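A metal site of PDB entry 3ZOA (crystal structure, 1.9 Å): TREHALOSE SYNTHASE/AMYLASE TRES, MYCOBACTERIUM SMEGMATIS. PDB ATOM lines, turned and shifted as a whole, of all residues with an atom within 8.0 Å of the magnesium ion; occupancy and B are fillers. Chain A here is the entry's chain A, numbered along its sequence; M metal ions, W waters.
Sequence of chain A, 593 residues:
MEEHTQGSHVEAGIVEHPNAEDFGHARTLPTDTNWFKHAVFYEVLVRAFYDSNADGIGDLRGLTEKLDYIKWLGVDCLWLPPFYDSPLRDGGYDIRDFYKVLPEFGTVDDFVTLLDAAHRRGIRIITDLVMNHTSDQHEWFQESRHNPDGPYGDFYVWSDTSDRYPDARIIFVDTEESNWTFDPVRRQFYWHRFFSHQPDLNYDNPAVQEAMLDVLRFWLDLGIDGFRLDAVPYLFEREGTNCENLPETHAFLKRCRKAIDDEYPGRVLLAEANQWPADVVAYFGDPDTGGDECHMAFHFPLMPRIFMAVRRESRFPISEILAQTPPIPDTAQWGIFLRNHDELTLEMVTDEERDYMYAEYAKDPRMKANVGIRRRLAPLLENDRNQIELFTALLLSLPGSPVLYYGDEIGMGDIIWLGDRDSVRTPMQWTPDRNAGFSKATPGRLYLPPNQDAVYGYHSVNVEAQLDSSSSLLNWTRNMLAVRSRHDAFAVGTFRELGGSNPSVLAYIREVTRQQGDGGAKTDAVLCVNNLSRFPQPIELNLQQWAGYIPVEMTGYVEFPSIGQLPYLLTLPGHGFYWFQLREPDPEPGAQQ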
ATOM      1  N   VAL A  46      24.564 -22.663 -11.066  1.00  0.00           N
ATOM      2  CA  VAL A  46      24.072 -21.437 -10.457  1.00  0.00           C
ATOM      3  C   VAL A  46      23.236 -20.651 -11.467  1.00  0.00           C
ATOM      4  O   VAL A  46      22.170 -20.155 -11.122  1.00  0.00           O
ATOM      5  CB  VAL A  46      25.248 -20.575  -9.962  1.00  0.00           C
ATOM      6  CG1 VAL A  46      24.721 -19.227  -9.444  1.00  0.00           C
ATOM      7  CG2 VAL A  46      25.994 -21.327  -8.856  1.00  0.00           C
ATOM      8  N   ARG A  47      23.696 -20.546 -12.706  1.00  0.00           N
ATOM      9  CA  ARG A  47      22.985 -19.703 -13.679  1.00  0.00           C
ATOM     10  C   ARG A  47      21.585 -20.218 -13.978  1.00  0.00           C
ATOM     11  O   ARG A  47      20.707 -19.446 -14.386  1.00  0.00           O
ATOM     12  CB  ARG A  47      23.789 -19.615 -14.996  1.00  0.00           C
ATOM     13  CG  ARG A  47      23.707 -20.896 -15.839  1.00  0.00           C
ATOM     14  CD  ARG A  47      24.578 -20.814 -17.107  1.00  0.00           C
ATOM     15  NE  ARG A  47      26.001 -20.811 -16.789  1.00  0.00           N
ATOM     16  CZ  ARG A  47      26.971 -21.201 -17.616  1.00  0.00           C
ATOM     17  NH1 ARG A  47      26.669 -21.623 -18.833  1.00  0.00           N
ATOM     18  NH2 ARG A  47      28.242 -21.169 -17.227  1.00  0.00           N
ATOM     19  N   TYR A  50      17.752 -20.693 -10.060  1.00  0.00           N
ATOM     20  CA  TYR A  50      16.731 -19.733  -9.678  1.00  0.00           C
ATOM     21  C   TYR A  50      17.250 -18.307  -9.714  1.00  0.00           C
ATOM     22  O   TYR A  50      18.270 -17.987  -9.111  1.00  0.00           O
ATOM     23  CB  TYR A  50      16.153 -20.073  -8.303  1.00  0.00           C
ATOM     24  CG  TYR A  50      14.959 -19.215  -7.954  1.00  0.00           C
ATOM     25  CD1 TYR A  50      13.824 -19.214  -8.757  1.00  0.00           C
ATOM     26  CD2 TYR A  50      14.978 -18.406  -6.825  1.00  0.00           C
ATOM     27  CE1 TYR A  50      12.739 -18.416  -8.440  1.00  0.00           C
ATOM     28  CE2 TYR A  50      13.902 -17.608  -6.509  1.00  0.00           C
ATOM     29  CZ  TYR A  50      12.787 -17.619  -7.320  1.00  0.00           C
ATOM     30  OH  TYR A  50      11.713 -16.826  -6.991  1.00  0.00           O
ATOM     31  N   ASP A  51      16.549 -17.452 -10.453  1.00  0.00           N
ATOM     32  CA  ASP A  51      16.903 -16.036 -10.586  1.00  0.00           C
ATOM     33  C   ASP A  51      16.133 -15.208  -9.554  1.00  0.00           C
ATOM     34  O   ASP A  51      14.969 -14.884  -9.758  1.00  0.00           O
ATOM     35  CB  ASP A  51      16.547 -15.550 -11.986  1.00  0.00           C
ATOM     36  CG  ASP A  51      16.772 -14.069 -12.174  1.00  0.00           C
ATOM     37  OD1 ASP A  51      17.630 -13.499 -11.460  1.00  0.00           O
ATOM     38  OD2 ASP A  51      16.090 -13.461 -13.039  1.00  0.00           O
ATOM     39  N   SER A  52      16.792 -14.832  -8.460  1.00  0.00           N
ATOM     40  CA  SER A  52      16.101 -14.132  -7.383  1.00  0.00           C
ATOM     41  C   SER A  52      16.026 -12.629  -7.621  1.00  0.00           C
ATOM     42  O   SER A  52      15.307 -11.920  -6.906  1.00  0.00           O
ATOM     43  CB  SER A  52      16.825 -14.384  -6.063  1.00  0.00           C
ATOM     44  OG  SER A  52      18.059 -13.694  -6.069  1.00  0.00           O
ATOM     45  N   ASN A  53      16.785 -12.107  -8.593  1.00  0.00           N
ATOM     46  CA  ASN A  53      16.862 -10.648  -8.754  1.00  0.00           C
ATOM     47  C   ASN A  53      16.345 -10.107 -10.070  1.00  0.00           C
ATOM     48  O   ASN A  53      16.587  -8.938 -10.412  1.00  0.00           O
ATOM     49  CB  ASN A  53      18.272 -10.133  -8.456  1.00  0.00           C
ATOM     50  CG  ASN A  53      19.340 -10.755  -9.338  1.00  0.00           C
ATOM     51  OD1 ASN A  53      19.025 -11.426 -10.315  1.00  0.00           O
ATOM     52  ND2 ASN A  53      20.603 -10.541  -8.981  1.00  0.00           N
ATOM     53  N   ALA A  54      15.631 -10.960 -10.812  1.00  0.00           N
ATOM     54  CA  ALA A  54      14.955 -10.574 -12.054  1.00  0.00           C
ATOM     55  C   ALA A  54      15.851  -9.959 -13.114  1.00  0.00           C
ATOM     56  O   ALA A  54      15.430  -9.068 -13.869  1.00  0.00           O
ATOM     57  CB  ALA A  54      13.753  -9.651 -11.754  1.00  0.00           C
ATOM     58  N   ASP A  55      17.091 -10.433 -13.205  1.00  0.00           N
ATOM     59  CA  ASP A  55      17.957 -10.018 -14.297  1.00  0.00           C
ATOM     60  C   ASP A  55      17.990 -11.085 -15.377  1.00  0.00           C
ATOM     61  O   ASP A  55      18.683 -10.939 -16.378  1.00  0.00           O
ATOM     62  CB  ASP A  55      19.366  -9.673 -13.806  1.00  0.00           C
ATOM     63  CG  ASP A  55      20.106 -10.854 -13.207  1.00  0.00           C
ATOM     64  OD1 ASP A  55      19.493 -11.930 -12.991  1.00  0.00           O
ATOM     65  OD2 ASP A  55      21.320 -10.708 -12.925  1.00  0.00           O
ATOM     66  N   GLY A  56      17.233 -12.158 -15.178  1.00  0.00           N
ATOM     67  CA  GLY A  56      17.147 -13.219 -16.170  1.00  0.00           C
ATOM     68  C   GLY A  56      18.217 -14.289 -15.964  1.00  0.00           C
ATOM     69  O   GLY A  56      18.280 -15.251 -16.721  1.00  0.00           O
ATOM     70  N   ILE A  57      19.044 -14.121 -14.933  1.00  0.00           N
ATOM     71  CA  ILE A  57      20.163 -15.039 -14.711  1.00  0.00           C
ATOM     72  C   ILE A  57      20.098 -15.634 -13.312  1.00  0.00           C
ATOM     73  O   ILE A  57      19.906 -14.907 -12.340  1.00  0.00           O
ATOM     74  CB  ILE A  57      21.518 -14.320 -14.876  1.00  0.00           C
ATOM     75  CG1 ILE A  57      21.547 -13.537 -16.209  1.00  0.00           C
ATOM     76  CG2 ILE A  57      22.668 -15.325 -14.817  1.00  0.00           C
ATOM     77  CD1 ILE A  57      22.718 -12.571 -16.348  1.00  0.00           C
ATOM     78  N   GLY A  58      20.252 -16.947 -13.208  1.00  0.00           N
ATOM     79  CA  GLY A  58      20.225 -17.602 -11.908  1.00  0.00           C
ATOM     80  C   GLY A  58      21.362 -17.046 -11.070  1.00  0.00           C
ATOM     81  O   GLY A  58      22.381 -16.593 -11.605  1.00  0.00           O
ATOM     82  N   ASP A  59      21.202 -17.063  -9.752  1.00  0.00           N
ATOM     83  CA  ASP A  59      22.199 -16.442  -8.891  1.00  0.00           C
ATOM     84  C   ASP A  59      22.338 -17.185  -7.574  1.00  0.00           C
ATOM     85  O   ASP A  59      21.543 -18.078  -7.250  1.00  0.00           O
ATOM     86  CB  ASP A  59      21.841 -14.968  -8.677  1.00  0.00           C
ATOM     87  CG  ASP A  59      20.346 -14.749  -8.501  1.00  0.00           C
ATOM     88  OD1 ASP A  59      19.819 -15.162  -7.441  1.00  0.00           O
ATOM     89  OD2 ASP A  59      19.706 -14.190  -9.438  1.00  0.00           O
ATOM     90  N   LEU A  60      23.389 -16.863  -6.811  1.00  0.00           N
ATOM     91  CA  LEU A  60      23.659 -17.572  -5.568  1.00  0.00           C
ATOM     92  C   LEU A  60      22.537 -17.399  -4.554  1.00  0.00           C
ATOM     93  O   LEU A  60      22.162 -18.353  -3.882  1.00  0.00           O
ATOM     94  CB  LEU A  60      25.010 -17.128  -4.959  1.00  0.00           C
ATOM     95  CG  LEU A  60      26.253 -17.514  -5.777  1.00  0.00           C
ATOM     96  CD1 LEU A  60      27.483 -16.742  -5.272  1.00  0.00           C
ATOM     97  CD2 LEU A  60      26.505 -19.029  -5.731  1.00  0.00           C
ATOM     98  N   ARG A  61      22.001 -16.186  -4.437  1.00  0.00           N
ATOM     99  CA  ARG A  61      20.882 -15.955  -3.546  1.00  0.00           C
ATOM    100  C   ARG A  61      19.671 -16.816  -3.928  1.00  0.00           C
ATOM    101  O   ARG A  61      18.979 -17.366  -3.063  1.00  0.00           O
ATOM    102  CB  ARG A  61      20.500 -14.474  -3.518  1.00  0.00           C
ATOM    103  CG  ARG A  61      19.319 -14.159  -2.623  1.00  0.00           C
ATOM    104  CD  ARG A  61      19.358 -12.687  -2.150  1.00  0.00           C
ATOM    105  NE  ARG A  61      20.438 -12.463  -1.185  1.00  0.00           N
ATOM    106  CZ  ARG A  61      20.617 -11.341  -0.481  1.00  0.00           C
ATOM    107  NH1 ARG A  61      19.768 -10.326  -0.625  1.00  0.00           N
ATOM    108  NH2 ARG A  61      21.634 -11.244   0.371  1.00  0.00           N
ATOM    109  N   GLY A  62      19.452 -16.953  -5.232  1.00  0.00           N
ATOM    110  CA  GLY A  62      18.364 -17.772  -5.746  1.00  0.00           C
ATOM    111  C   GLY A  62      18.556 -19.232  -5.377  1.00  0.00           C
ATOM    112  O   GLY A  62      17.618 -19.896  -4.946  1.00  0.00           O
ATOM    113  N   GLU A 104      27.356 -11.433 -12.027  1.00  0.00           N
ATOM    114  CA  GLU A 104      25.916 -11.635 -12.115  1.00  0.00           C
ATOM    115  C   GLU A 104      25.397 -12.730 -11.181  1.00  0.00           C
ATOM    116  O   GLU A 104      24.195 -12.849 -10.983  1.00  0.00           O
ATOM    117  CB  GLU A 104      25.450 -11.869 -13.555  1.00  0.00           C
ATOM    118  CG  GLU A 104      26.047 -13.073 -14.209  1.00  0.00           C
ATOM    119  CD  GLU A 104      26.553 -12.733 -15.597  1.00  0.00           C
ATOM    120  OE1 GLU A 104      27.240 -11.690 -15.721  1.00  0.00           O
ATOM    121  OE2 GLU A 104      26.284 -13.509 -16.546  1.00  0.00           O
ATOM    122  N   PHE A 105      26.299 -13.513 -10.595  1.00  0.00           N
ATOM    123  CA  PHE A 105      25.895 -14.525  -9.612  1.00  0.00           C
ATOM    124  C   PHE A 105      25.868 -13.977  -8.190  1.00  0.00           C
ATOM    125  O   PHE A 105      25.219 -14.550  -7.309  1.00  0.00           O
ATOM    126  CB  PHE A 105      26.834 -15.732  -9.660  1.00  0.00           C
ATOM    127  CG  PHE A 105      26.764 -16.510 -10.938  1.00  0.00           C
ATOM    128  CD1 PHE A 105      25.679 -16.391 -11.809  1.00  0.00           C
ATOM    129  CD2 PHE A 105      27.787 -17.379 -11.283  1.00  0.00           C
ATOM    130  CE1 PHE A 105      25.621 -17.117 -12.991  1.00  0.00           C
ATOM    131  CE2 PHE A 105      27.750 -18.113 -12.464  1.00  0.00           C
ATOM    132  CZ  PHE A 105      26.656 -17.978 -13.319  1.00  0.00           C
ATOM    133  N   GLY A 106      26.582 -12.886  -7.944  1.00  0.00           N
ATOM    134  CA  GLY A 106      26.705 -12.340  -6.605  1.00  0.00           C
ATOM    135  C   GLY A 106      28.187 -12.153  -6.275  1.00  0.00           C
ATOM    136  O   GLY A 106      28.992 -11.993  -7.185  1.00  0.00           O
ATOM    137  N   PHE A 438      11.187 -19.660 -13.169  1.00  0.00           N
ATOM    138  CA  PHE A 438      12.613 -19.498 -12.886  1.00  0.00           C
ATOM    139  C   PHE A 438      12.988 -18.035 -12.626  1.00  0.00           C
ATOM    140  O   PHE A 438      13.934 -17.734 -11.896  1.00  0.00           O
ATOM    141  CB  PHE A 438      13.411 -20.087 -14.056  1.00  0.00           C
ATOM    142  CG  PHE A 438      14.803 -19.526 -14.191  1.00  0.00           C
ATOM    143  CD1 PHE A 438      15.854 -20.010 -13.412  1.00  0.00           C
ATOM    144  CD2 PHE A 438      15.070 -18.519 -15.134  1.00  0.00           C
ATOM    145  CE1 PHE A 438      17.136 -19.491 -13.549  1.00  0.00           C
ATOM    146  CE2 PHE A 438      16.351 -17.994 -15.284  1.00  0.00           C
ATOM    147  CZ  PHE A 438      17.385 -18.468 -14.475  1.00  0.00           C
ATOM    148  N   SER A 439      12.233 -17.114 -13.222  1.00  0.00           N
ATOM    149  CA  SER A 439      12.585 -15.698 -13.147  1.00  0.00           C
ATOM    150  C   SER A 439      11.362 -14.824 -13.326  1.00  0.00           C
ATOM    151  O   SER A 439      10.408 -15.234 -13.976  1.00  0.00           O
ATOM    152  CB  SER A 439      13.579 -15.368 -14.283  1.00  0.00           C
ATOM    153  OG  SER A 439      13.884 -13.975 -14.334  1.00  0.00           O
ATOM    154  N   ALA A 441      11.920 -11.865 -14.798  1.00  0.00           N
ATOM    155  CA  ALA A 441      12.363 -10.990 -15.882  1.00  0.00           C
ATOM    156  C   ALA A 441      11.528 -11.242 -17.138  1.00  0.00           C
ATOM    157  O   ALA A 441      10.754 -12.198 -17.205  1.00  0.00           O
ATOM    158  CB  ALA A 441      13.851 -11.210 -16.188  1.00  0.00           C
HETATM  159 MG    MG M   1      19.636 -13.197 -11.264  1.00  0.00          MG
HETATM  160  O   HOH W   1      21.694 -12.664 -11.250  1.00  0.00           O
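Within 4 Å of the magnesium ion: Asp 51, Asn 53, Asp 55, Ile 57 and Asp 59.
Along chain A the residues within 4 Å of the magnesium ion span positions 51 to 59.
The nearest printed residue that does not touch the magnesium ion is Gly 58 (4.2 Å).
The backbone NH of Ala 54 lies close to the side-chain carboxylate of Asp 51.
The side-chain carboxylate (OD2) of Asp 51 lies within hydrogen-bond range of the backbone NH (N) of Gly 56 (2.8 Å).
The side-chain carboxylate of Asp 51 is in hydrogen-bond range of the side-chain hydroxyl of Ser 439, 2.6 Å away.
O of Phe 438 sits at hydrogen-bond distance from N of Asp 51, at 3.0 Å.
OG of Ser 52 lies within hydrogen-bond range of OD1 of Asp 59 (2.7 Å).
N of Asp 59 is in hydrogen-bond range of O of Tyr 50 (3.1 Å).
OD1 of Asp 59 is in hydrogen-bond range of N of Gly 62 (2.9 Å).
O of Ile 57 is bound to the magnesium ion, 2.0 Å away.
The magnesium ion is bound by the side-chain carboxylate (OD1) of Asp 51, at 2.0 Å.
The side-chain carboxylate (OD2) of Asp 59 is bound to the magnesium ion, 2.1 Å away.
The magnesium ion is bound by OD1 of Asn 53 (2.1 Å).
The magnesium ion is bound by water W1, 2.1 Å away.
The magnesium ion is bound by OD1 of Asp 55, 2.1 Å away.
The magnesium ion has six donor atoms within binding distance.
Water W1 lies within hydrogen-bond range of O of Glu 104 (2.5 Å), OD2 of Asp 55 (2.6 Å) and ND2 of Asn 53 (3.3 Å).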
